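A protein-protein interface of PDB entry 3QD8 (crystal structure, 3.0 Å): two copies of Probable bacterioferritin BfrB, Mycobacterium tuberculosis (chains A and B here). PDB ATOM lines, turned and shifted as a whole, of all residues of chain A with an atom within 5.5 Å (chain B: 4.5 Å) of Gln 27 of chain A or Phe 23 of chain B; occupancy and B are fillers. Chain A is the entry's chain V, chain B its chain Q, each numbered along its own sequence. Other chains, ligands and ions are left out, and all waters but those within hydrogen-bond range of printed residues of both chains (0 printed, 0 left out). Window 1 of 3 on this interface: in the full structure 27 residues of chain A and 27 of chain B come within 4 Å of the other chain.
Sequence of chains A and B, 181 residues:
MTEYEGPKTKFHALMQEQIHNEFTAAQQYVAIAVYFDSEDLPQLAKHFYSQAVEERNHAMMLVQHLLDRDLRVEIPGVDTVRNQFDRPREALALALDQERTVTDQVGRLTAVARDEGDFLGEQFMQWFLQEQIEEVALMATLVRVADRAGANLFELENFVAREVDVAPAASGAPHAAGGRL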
ATOM      1  N   GLU A  22     -28.733  -7.802  -3.171  1.00  0.00           N
ATOM      2  CA  GLU A  22     -29.287  -6.852  -4.123  1.00  0.00           C
ATOM      3  C   GLU A  22     -28.179  -6.029  -4.797  1.00  0.00           C
ATOM      4  O   GLU A  22     -28.160  -5.892  -6.021  1.00  0.00           O
ATOM      5  CB  GLU A  22     -30.344  -5.948  -3.457  1.00  0.00           C
ATOM      6  CG  GLU A  22     -31.537  -6.703  -2.871  1.00  0.00           C
ATOM      7  CD  GLU A  22     -32.635  -6.971  -3.873  1.00  0.00           C
ATOM      8  OE1 GLU A  22     -32.369  -6.946  -5.092  1.00  0.00           O
ATOM      9  OE2 GLU A  22     -33.772  -7.214  -3.430  1.00  0.00           O
ATOM     10  N   PHE A  23     -27.253  -5.479  -4.018  1.00  0.00           N
ATOM     11  CA  PHE A  23     -26.172  -4.727  -4.639  1.00  0.00           C
ATOM     12  C   PHE A  23     -25.463  -5.594  -5.664  1.00  0.00           C
ATOM     13  O   PHE A  23     -25.133  -5.121  -6.748  1.00  0.00           O
ATOM     14  CB  PHE A  23     -25.171  -4.188  -3.614  1.00  0.00           C
ATOM     15  CG  PHE A  23     -25.537  -2.856  -3.057  1.00  0.00           C
ATOM     16  CD1 PHE A  23     -25.488  -1.724  -3.852  1.00  0.00           C
ATOM     17  CD2 PHE A  23     -25.916  -2.727  -1.743  1.00  0.00           C
ATOM     18  CE1 PHE A  23     -25.830  -0.477  -3.343  1.00  0.00           C
ATOM     19  CE2 PHE A  23     -26.248  -1.486  -1.226  1.00  0.00           C
ATOM     20  CZ  PHE A  23     -26.208  -0.361  -2.031  1.00  0.00           C
ATOM     21  N   THR A  24     -25.233  -6.857  -5.315  1.00  0.00           N
ATOM     22  CA  THR A  24     -24.605  -7.803  -6.228  1.00  0.00           C
ATOM     23  C   THR A  24     -25.440  -8.050  -7.478  1.00  0.00           C
ATOM     24  O   THR A  24     -24.948  -7.958  -8.606  1.00  0.00           O
ATOM     25  CB  THR A  24     -24.377  -9.137  -5.544  1.00  0.00           C
ATOM     26  OG1 THR A  24     -23.216  -9.033  -4.718  1.00  0.00           O
ATOM     27  CG2 THR A  24     -24.170 -10.218  -6.574  1.00  0.00           C
ATOM     28  N   ALA A  25     -26.708  -8.381  -7.264  1.00  0.00           N
ATOM     29  CA  ALA A  25     -27.651  -8.567  -8.355  1.00  0.00           C
ATOM     30  C   ALA A  25     -27.609  -7.379  -9.315  1.00  0.00           C
ATOM     31  O   ALA A  25     -27.523  -7.541 -10.536  1.00  0.00           O
ATOM     32  CB  ALA A  25     -29.029  -8.738  -7.808  1.00  0.00           C
ATOM     33  N   ALA A  26     -27.672  -6.175  -8.755  1.00  0.00           N
ATOM     34  CA  ALA A  26     -27.663  -4.958  -9.558  1.00  0.00           C
ATOM     35  C   ALA A  26     -26.393  -4.871 -10.398  1.00  0.00           C
ATOM     36  O   ALA A  26     -26.446  -4.581 -11.596  1.00  0.00           O
ATOM     37  CB  ALA A  26     -27.811  -3.734  -8.668  1.00  0.00           C
ATOM     38  N   GLN A  27     -25.252  -5.136  -9.770  1.00  0.00           N
ATOM     39  CA  GLN A  27     -23.974  -5.117 -10.475  1.00  0.00           C
ATOM     40  C   GLN A  27     -24.027  -6.084 -11.645  1.00  0.00           C
ATOM     41  O   GLN A  27     -23.575  -5.750 -12.744  1.00  0.00           O
ATOM     42  CB  GLN A  27     -22.804  -5.478  -9.548  1.00  0.00           C
ATOM     43  CG  GLN A  27     -21.440  -5.072 -10.092  1.00  0.00           C
ATOM     44  CD  GLN A  27     -21.239  -3.552 -10.128  1.00  0.00           C
ATOM     45  OE1 GLN A  27     -22.182  -2.779  -9.899  1.00  0.00           O
ATOM     46  NE2 GLN A  27     -20.005  -3.120 -10.413  1.00  0.00           N
ATOM     47  N   GLN A  28     -24.594  -7.271 -11.406  1.00  0.00           N
ATOM     48  CA  GLN A  28     -24.662  -8.303 -12.433  1.00  0.00           C
ATOM     49  C   GLN A  28     -25.438  -7.810 -13.645  1.00  0.00           C
ATOM     50  O   GLN A  28     -25.116  -8.155 -14.789  1.00  0.00           O
ATOM     51  CB  GLN A  28     -25.275  -9.589 -11.876  1.00  0.00           C
ATOM     52  CG  GLN A  28     -25.500 -10.687 -12.931  1.00  0.00           C
ATOM     53  CD  GLN A  28     -24.214 -11.168 -13.618  1.00  0.00           C
ATOM     54  OE1 GLN A  28     -23.454 -11.983 -13.070  1.00  0.00           O
ATOM     55  NE2 GLN A  28     -23.979 -10.676 -14.830  1.00  0.00           N
ATOM     56  N   TYR A  29     -26.455  -6.993 -13.383  1.00  0.00           N
ATOM     57  CA  TYR A  29     -27.228  -6.379 -14.452  1.00  0.00           C
ATOM     58  C   TYR A  29     -26.372  -5.427 -15.288  1.00  0.00           C
ATOM     59  O   TYR A  29     -26.399  -5.476 -16.523  1.00  0.00           O
ATOM     60  CB  TYR A  29     -28.451  -5.648 -13.896  1.00  0.00           C
ATOM     61  CG  TYR A  29     -29.638  -6.546 -13.650  1.00  0.00           C
ATOM     62  CD1 TYR A  29     -29.840  -7.694 -14.414  1.00  0.00           C
ATOM     63  CD2 TYR A  29     -30.567  -6.247 -12.662  1.00  0.00           C
ATOM     64  CE1 TYR A  29     -30.932  -8.523 -14.187  1.00  0.00           C
ATOM     65  CE2 TYR A  29     -31.663  -7.070 -12.432  1.00  0.00           C
ATOM     66  CZ  TYR A  29     -31.837  -8.199 -13.194  1.00  0.00           C
ATOM     67  OH  TYR A  29     -32.921  -9.002 -12.965  1.00  0.00           O
ATOM     68  N   VAL A  30     -25.616  -4.557 -14.622  1.00  0.00           N
ATOM     69  CA  VAL A  30     -24.705  -3.679 -15.346  1.00  0.00           C
ATOM     70  C   VAL A  30     -23.826  -4.529 -16.290  1.00  0.00           C
ATOM     71  O   VAL A  30     -23.648  -4.218 -17.475  1.00  0.00           O
ATOM     72  CB  VAL A  30     -23.817  -2.874 -14.391  1.00  0.00           C
ATOM     73  CG1 VAL A  30     -23.061  -1.819 -15.174  1.00  0.00           C
ATOM     74  CG2 VAL A  30     -24.643  -2.246 -13.305  1.00  0.00           C
ATOM     75  N   ALA A  31     -23.287  -5.615 -15.746  1.00  0.00           N
ATOM     76  CA  ALA A  31     -22.457  -6.519 -16.511  1.00  0.00           C
ATOM     77  C   ALA A  31     -23.202  -6.987 -17.750  1.00  0.00           C
ATOM     78  O   ALA A  31     -22.711  -6.854 -18.875  1.00  0.00           O
ATOM     79  CB  ALA A  31     -22.052  -7.693 -15.658  1.00  0.00           C
ATOM     80  N   ILE A  32     -24.390  -7.530 -17.537  1.00  0.00           N
ATOM     81  CA  ILE A  32     -25.240  -7.929 -18.640  1.00  0.00           C
ATOM     82  C   ILE A  32     -25.536  -6.771 -19.609  1.00  0.00           C
ATOM     83  O   ILE A  32     -25.509  -6.955 -20.824  1.00  0.00           O
ATOM     84  CB  ILE A  32     -26.551  -8.528 -18.124  1.00  0.00           C
ATOM     85  CG1 ILE A  32     -26.257  -9.813 -17.364  1.00  0.00           C
ATOM     86  CG2 ILE A  32     -27.539  -8.758 -19.292  1.00  0.00           C
ATOM     87  CD1 ILE A  32     -27.451 -10.430 -16.736  1.00  0.00           C
ATOM     88  N   VAL A  78     -19.291  -5.880  -3.146  1.00  0.00           N
ATOM     89  CA  VAL A  78     -20.056  -6.617  -4.135  1.00  0.00           C
ATOM     90  C   VAL A  78     -19.216  -7.717  -4.764  1.00  0.00           C
ATOM     91  O   VAL A  78     -18.075  -7.486  -5.157  1.00  0.00           O
ATOM     92  CB  VAL A  78     -20.574  -5.677  -5.229  1.00  0.00           C
ATOM     93  CG1 VAL A  78     -21.535  -6.415  -6.138  1.00  0.00           C
ATOM     94  CG2 VAL A  78     -21.244  -4.463  -4.604  1.00  0.00           C
ATOM     95  N   ASP A  79     -19.781  -8.917  -4.855  1.00  0.00           N
ATOM     96  CA  ASP A  79     -19.046 -10.064  -5.383  1.00  0.00           C
ATOM     97  C   ASP A  79     -18.754  -9.894  -6.857  1.00  0.00           C
ATOM     98  O   ASP A  79     -19.452  -9.156  -7.543  1.00  0.00           O
ATOM     99  CB  ASP A  79     -19.854 -11.338  -5.183  1.00  0.00           C
ATOM    100  CG  ASP A  79     -20.081 -11.648  -3.728  1.00  0.00           C
ATOM    101  OD1 ASP A  79     -19.166 -11.362  -2.921  1.00  0.00           O
ATOM    102  OD2 ASP A  79     -21.170 -12.173  -3.397  1.00  0.00           O
ATOM    103  N   VAL A  81     -19.048 -10.481 -10.657  1.00  0.00           N
ATOM    104  CA  VAL A  81     -20.235 -10.901 -11.396  1.00  0.00           C
ATOM    105  C   VAL A  81     -19.789 -11.375 -12.760  1.00  0.00           C
ATOM    106  O   VAL A  81     -18.661 -11.122 -13.176  1.00  0.00           O
ATOM    107  CB  VAL A  81     -21.275  -9.769 -11.563  1.00  0.00           C
ATOM    108  CG1 VAL A  81     -21.712  -9.226 -10.203  1.00  0.00           C
ATOM    109  CG2 VAL A  81     -20.724  -8.659 -12.417  1.00  0.00           C
ATOM    110  N   ILE B  19     -11.854   1.324 -13.571  1.00  0.00           N
ATOM    111  CA  ILE B  19     -13.280   1.003 -13.509  1.00  0.00           C
ATOM    112  C   ILE B  19     -13.611   0.379 -12.158  1.00  0.00           C
ATOM    113  O   ILE B  19     -14.606   0.722 -11.519  1.00  0.00           O
ATOM    114  CB  ILE B  19     -13.695   0.023 -14.622  1.00  0.00           C
ATOM    115  CG1 ILE B  19     -13.638   0.727 -15.971  1.00  0.00           C
ATOM    116  CG2 ILE B  19     -15.078  -0.506 -14.367  1.00  0.00           C
ATOM    117  CD1 ILE B  19     -13.985  -0.143 -17.115  1.00  0.00           C
ATOM    118  N   HIS B  20     -12.763  -0.540 -11.717  1.00  0.00           N
ATOM    119  CA  HIS B  20     -12.949  -1.165 -10.419  1.00  0.00           C
ATOM    120  C   HIS B  20     -12.818  -0.125  -9.318  1.00  0.00           C
ATOM    121  O   HIS B  20     -13.676  -0.051  -8.430  1.00  0.00           O
ATOM    122  CB  HIS B  20     -11.934  -2.282 -10.212  1.00  0.00           C
ATOM    123  CG  HIS B  20     -11.903  -2.815  -8.816  1.00  0.00           C
ATOM    124  ND1 HIS B  20     -12.648  -3.902  -8.415  1.00  0.00           N
ATOM    125  CD2 HIS B  20     -11.224  -2.402  -7.719  1.00  0.00           C
ATOM    126  CE1 HIS B  20     -12.434  -4.136  -7.131  1.00  0.00           C
ATOM    127  NE2 HIS B  20     -11.574  -3.238  -6.684  1.00  0.00           N
ATOM    128  N   ASN B  21     -11.751   0.672  -9.374  1.00  0.00           N
ATOM    129  CA  ASN B  21     -11.519   1.691  -8.354  1.00  0.00           C
ATOM    130  C   ASN B  21     -12.720   2.620  -8.210  1.00  0.00           C
ATOM    131  O   ASN B  21     -13.186   2.899  -7.095  1.00  0.00           O
ATOM    132  CB  ASN B  21     -10.277   2.523  -8.676  1.00  0.00           C
ATOM    133  CG  ASN B  21      -9.011   1.710  -8.663  1.00  0.00           C
ATOM    134  OD1 ASN B  21      -8.980   0.598  -8.146  1.00  0.00           O
ATOM    135  ND2 ASN B  21      -7.955   2.261  -9.239  1.00  0.00           N
ATOM    136  N   GLU B  22     -13.213   3.100  -9.348  1.00  0.00           N
ATOM    137  CA  GLU B  22     -14.326   4.042  -9.347  1.00  0.00           C
ATOM    138  C   GLU B  22     -15.602   3.411  -8.773  1.00  0.00           C
ATOM    139  O   GLU B  22     -16.264   4.043  -7.944  1.00  0.00           O
ATOM    140  CB  GLU B  22     -14.569   4.617 -10.746  1.00  0.00           C
ATOM    141  CG  GLU B  22     -13.375   5.368 -11.335  1.00  0.00           C
ATOM    142  CD  GLU B  22     -13.348   6.827 -10.944  1.00  0.00           C
ATOM    143  OE1 GLU B  22     -13.932   7.157  -9.901  1.00  0.00           O
ATOM    144  OE2 GLU B  22     -12.753   7.648 -11.682  1.00  0.00           O
ATOM    145  N   PHE B  23     -15.949   2.185  -9.189  1.00  0.00           N
ATOM    146  CA  PHE B  23     -17.106   1.516  -8.608  1.00  0.00           C
ATOM    147  C   PHE B  23     -16.944   1.400  -7.097  1.00  0.00           C
ATOM    148  O   PHE B  23     -17.898   1.580  -6.346  1.00  0.00           O
ATOM    149  CB  PHE B  23     -17.297   0.138  -9.187  1.00  0.00           C
ATOM    150  CG  PHE B  23     -18.129   0.109 -10.423  1.00  0.00           C
ATOM    151  CD1 PHE B  23     -19.473   0.377 -10.366  1.00  0.00           C
ATOM    152  CD2 PHE B  23     -17.575  -0.220 -11.646  1.00  0.00           C
ATOM    153  CE1 PHE B  23     -20.250   0.360 -11.504  1.00  0.00           C
ATOM    154  CE2 PHE B  23     -18.349  -0.250 -12.782  1.00  0.00           C
ATOM    155  CZ  PHE B  23     -19.693   0.047 -12.709  1.00  0.00           C
ATOM    156  N   THR B  24     -15.729   1.095  -6.651  1.00  0.00           N
ATOM    157  CA  THR B  24     -15.440   1.034  -5.226  1.00  0.00           C
ATOM    158  C   THR B  24     -15.622   2.392  -4.569  1.00  0.00           C
ATOM    159  O   THR B  24     -16.360   2.525  -3.594  1.00  0.00           O
ATOM    160  CB  THR B  24     -14.014   0.567  -4.965  1.00  0.00           C
ATOM    161  OG1 THR B  24     -13.930  -0.858  -5.144  1.00  0.00           O
ATOM    162  CG2 THR B  24     -13.609   0.937  -3.543  1.00  0.00           C
ATOM    163  N   ALA B  25     -14.935   3.401  -5.102  1.00  0.00           N
ATOM    164  CA  ALA B  25     -15.042   4.768  -4.589  1.00  0.00           C
ATOM    165  C   ALA B  25     -16.496   5.171  -4.448  1.00  0.00           C
ATOM    166  O   ALA B  25     -16.895   5.717  -3.426  1.00  0.00           O
ATOM    167  CB  ALA B  25     -14.316   5.725  -5.507  1.00  0.00           C
ATOM    168  N   ALA B  26     -17.284   4.897  -5.487  1.00  0.00           N
ATOM    169  CA  ALA B  26     -18.700   5.252  -5.481  1.00  0.00           C
ATOM    170  C   ALA B  26     -19.411   4.556  -4.326  1.00  0.00           C
ATOM    171  O   ALA B  26     -20.205   5.184  -3.619  1.00  0.00           O
ATOM    172  CB  ALA B  26     -19.361   4.924  -6.809  1.00  0.00           C
ATOM    173  N   GLN B  27     -19.105   3.276  -4.118  1.00  0.00           N
ATOM    174  CA  GLN B  27     -19.755   2.512  -3.067  1.00  0.00           C
ATOM    175  C   GLN B  27     -19.445   3.147  -1.725  1.00  0.00           C
ATOM    176  O   GLN B  27     -20.323   3.280  -0.879  1.00  0.00           O
ATOM    177  CB  GLN B  27     -19.317   1.039  -3.094  1.00  0.00           C
ATOM    178  CG  GLN B  27     -20.206   0.098  -2.283  1.00  0.00           C
ATOM    179  CD  GLN B  27     -21.601  -0.082  -2.904  1.00  0.00           C
ATOM    180  OE1 GLN B  27     -21.942   0.548  -3.926  1.00  0.00           O
ATOM    181  NE2 GLN B  27     -22.406  -0.959  -2.296  1.00  0.00           N
ATOM    182  N   ALA B  59     -17.302   5.846 -13.523  1.00  0.00           N
ATOM    183  CA  ALA B  59     -17.068   4.457 -13.858  1.00  0.00           C
ATOM    184  C   ALA B  59     -17.667   4.149 -15.240  1.00  0.00           C
ATOM    185  O   ALA B  59     -16.964   3.710 -16.149  1.00  0.00           O
ATOM    186  CB  ALA B  59     -17.645   3.546 -12.785  1.00  0.00           C
ATOM    187  N   MET B  60     -18.952   4.415 -15.409  1.00  0.00           N
ATOM    188  CA  MET B  60     -19.612   4.130 -16.681  1.00  0.00           C
ATOM    189  C   MET B  60     -19.011   4.871 -17.882  1.00  0.00           C
ATOM    190  O   MET B  60     -19.101   4.392 -19.021  1.00  0.00           O
ATOM    191  CB  MET B  60     -21.123   4.375 -16.589  1.00  0.00           C
ATOM    192  CG  MET B  60     -21.774   3.550 -15.508  1.00  0.00           C
ATOM    193  SD  MET B  60     -21.325   1.814 -15.628  1.00  0.00           S
ATOM    194  CE  MET B  60     -22.477   1.307 -16.900  1.00  0.00           C
ATOM    195  N   ILE B  75     -17.268  -5.620 -15.919  1.00  0.00           N
ATOM    196  CA  ILE B  75     -17.865  -5.039 -14.725  1.00  0.00           C
ATOM    197  C   ILE B  75     -17.369  -5.813 -13.510  1.00  0.00           C
ATOM    198  O   ILE B  75     -17.702  -6.979 -13.329  1.00  0.00           O
ATOM    199  CB  ILE B  75     -19.397  -5.061 -14.784  1.00  0.00           C
ATOM    200  CG1 ILE B  75     -19.872  -4.366 -16.051  1.00  0.00           C
ATOM    201  CG2 ILE B  75     -19.978  -4.353 -13.580  1.00  0.00           C
ATOM    202  CD1 ILE B  75     -19.451  -2.922 -16.138  1.00  0.00           C
ATOM    203  N   PRO B  76     -16.566  -5.160 -12.668  1.00  0.00           N
ATOM    204  CA  PRO B  76     -15.883  -5.799 -11.540  1.00  0.00           C
ATOM    205  C   PRO B  76     -16.781  -5.937 -10.338  1.00  0.00           C
ATOM    206  O   PRO B  76     -17.869  -5.361 -10.309  1.00  0.00           O
ATOM    207  CB  PRO B  76     -14.798  -4.782 -11.168  1.00  0.00           C
ATOM    208  CG  PRO B  76     -15.111  -3.505 -11.957  1.00  0.00           C
ATOM    209  CD  PRO B  76     -16.434  -3.694 -12.630  1.00  0.00           C
ATOM    210  N   VAL B  78     -16.828  -5.205  -6.075  1.00  0.00           N
ATOM    211  CA  VAL B  78     -16.484  -4.004  -5.319  1.00  0.00           C
ATOM    212  C   VAL B  78     -15.996  -4.376  -3.941  1.00  0.00           C
ATOM    213  O   VAL B  78     -16.623  -5.175  -3.268  1.00  0.00           O
ATOM    214  CB  VAL B  78     -17.688  -3.065  -5.180  1.00  0.00           C
ATOM    215  CG1 VAL B  78     -17.267  -1.767  -4.499  1.00  0.00           C
ATOM    216  CG2 VAL B  78     -18.289  -2.799  -6.555  1.00  0.00           C
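Among the printed residues, pairs that only touch across the chains: Ala 31 of chain A with Ile 75 of chain B, Gln 27 of chain A with Ile 75 of chain B, Phe 23 of chain A with Gln 27 of chain B, Gln 27 of chain A with Phe 23 of chain B, Val 81 of chain A with Ile 75 of chain B, Val 30 of chain A with Met 60 of chain B and Val 30 of chain A with Ile 75 of chain B.
The backbone NH (N) of Val 78 of chain B sits at hydrogen-bond distance from the backbone carbonyl oxygen (O) of Val 78 of chain A, 2.8 Å away. NE2 of Gln 27 of chain A sits at hydrogen-bond distance from O of Pro 76 of chain B (3.1 Å).
Phe 23 of chain A touches Gln 27 of chain B, and with the chains exchanged Gln 27 of chain A touches Phe 23 of chain B. Val 78 of chain B touches its own counterpart, Val 78 of chain A. Of the 9 pairs that touch across the chains among the printed residues, 3 have their exchanged pair printed and touching as well.
Printed residues of chain B within 4 Å of Gln 27 of chain A: Phe 23 (3.5 Å), Ile 75 (3.4 Å) and Pro 76 (3.1 Å). Of chain A, only Gln 27 (3.5 Å) comes within 4 Å of Phe 23 of chain B. Printed residues of chain B within 4 Å of Val 81 of chain A: Ile 75. Printed residues of chain B within 4 Å of Val 30 of chain A: Met 60 (3.6 Å) and Ile 75 (3.9 Å). Ala 25 of chain B touches none of the printed residues of chain A. Ala 26 of chain A touches none of the printed residues of chain B. The nearest residue of chain B that does not touch Gln 27 of chain A is Val 78 of chain B (4.2 Å). The nearest residue of chain A that does not touch Phe 23 of chain B is Val 30 of chain A (4.6 Å).
Printed residues of chain A that touch a printed residue of chain B: Phe 23, Gln 27, Val 30, Ala 31, Val 78 and Val 81. Hydrophobic or aromatic side chains of chain B that line the printed part of chain A: Phe 23, Met 60, Ile 75 and Val 78. Among the printed residues, 9 pairs touch across the chains.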
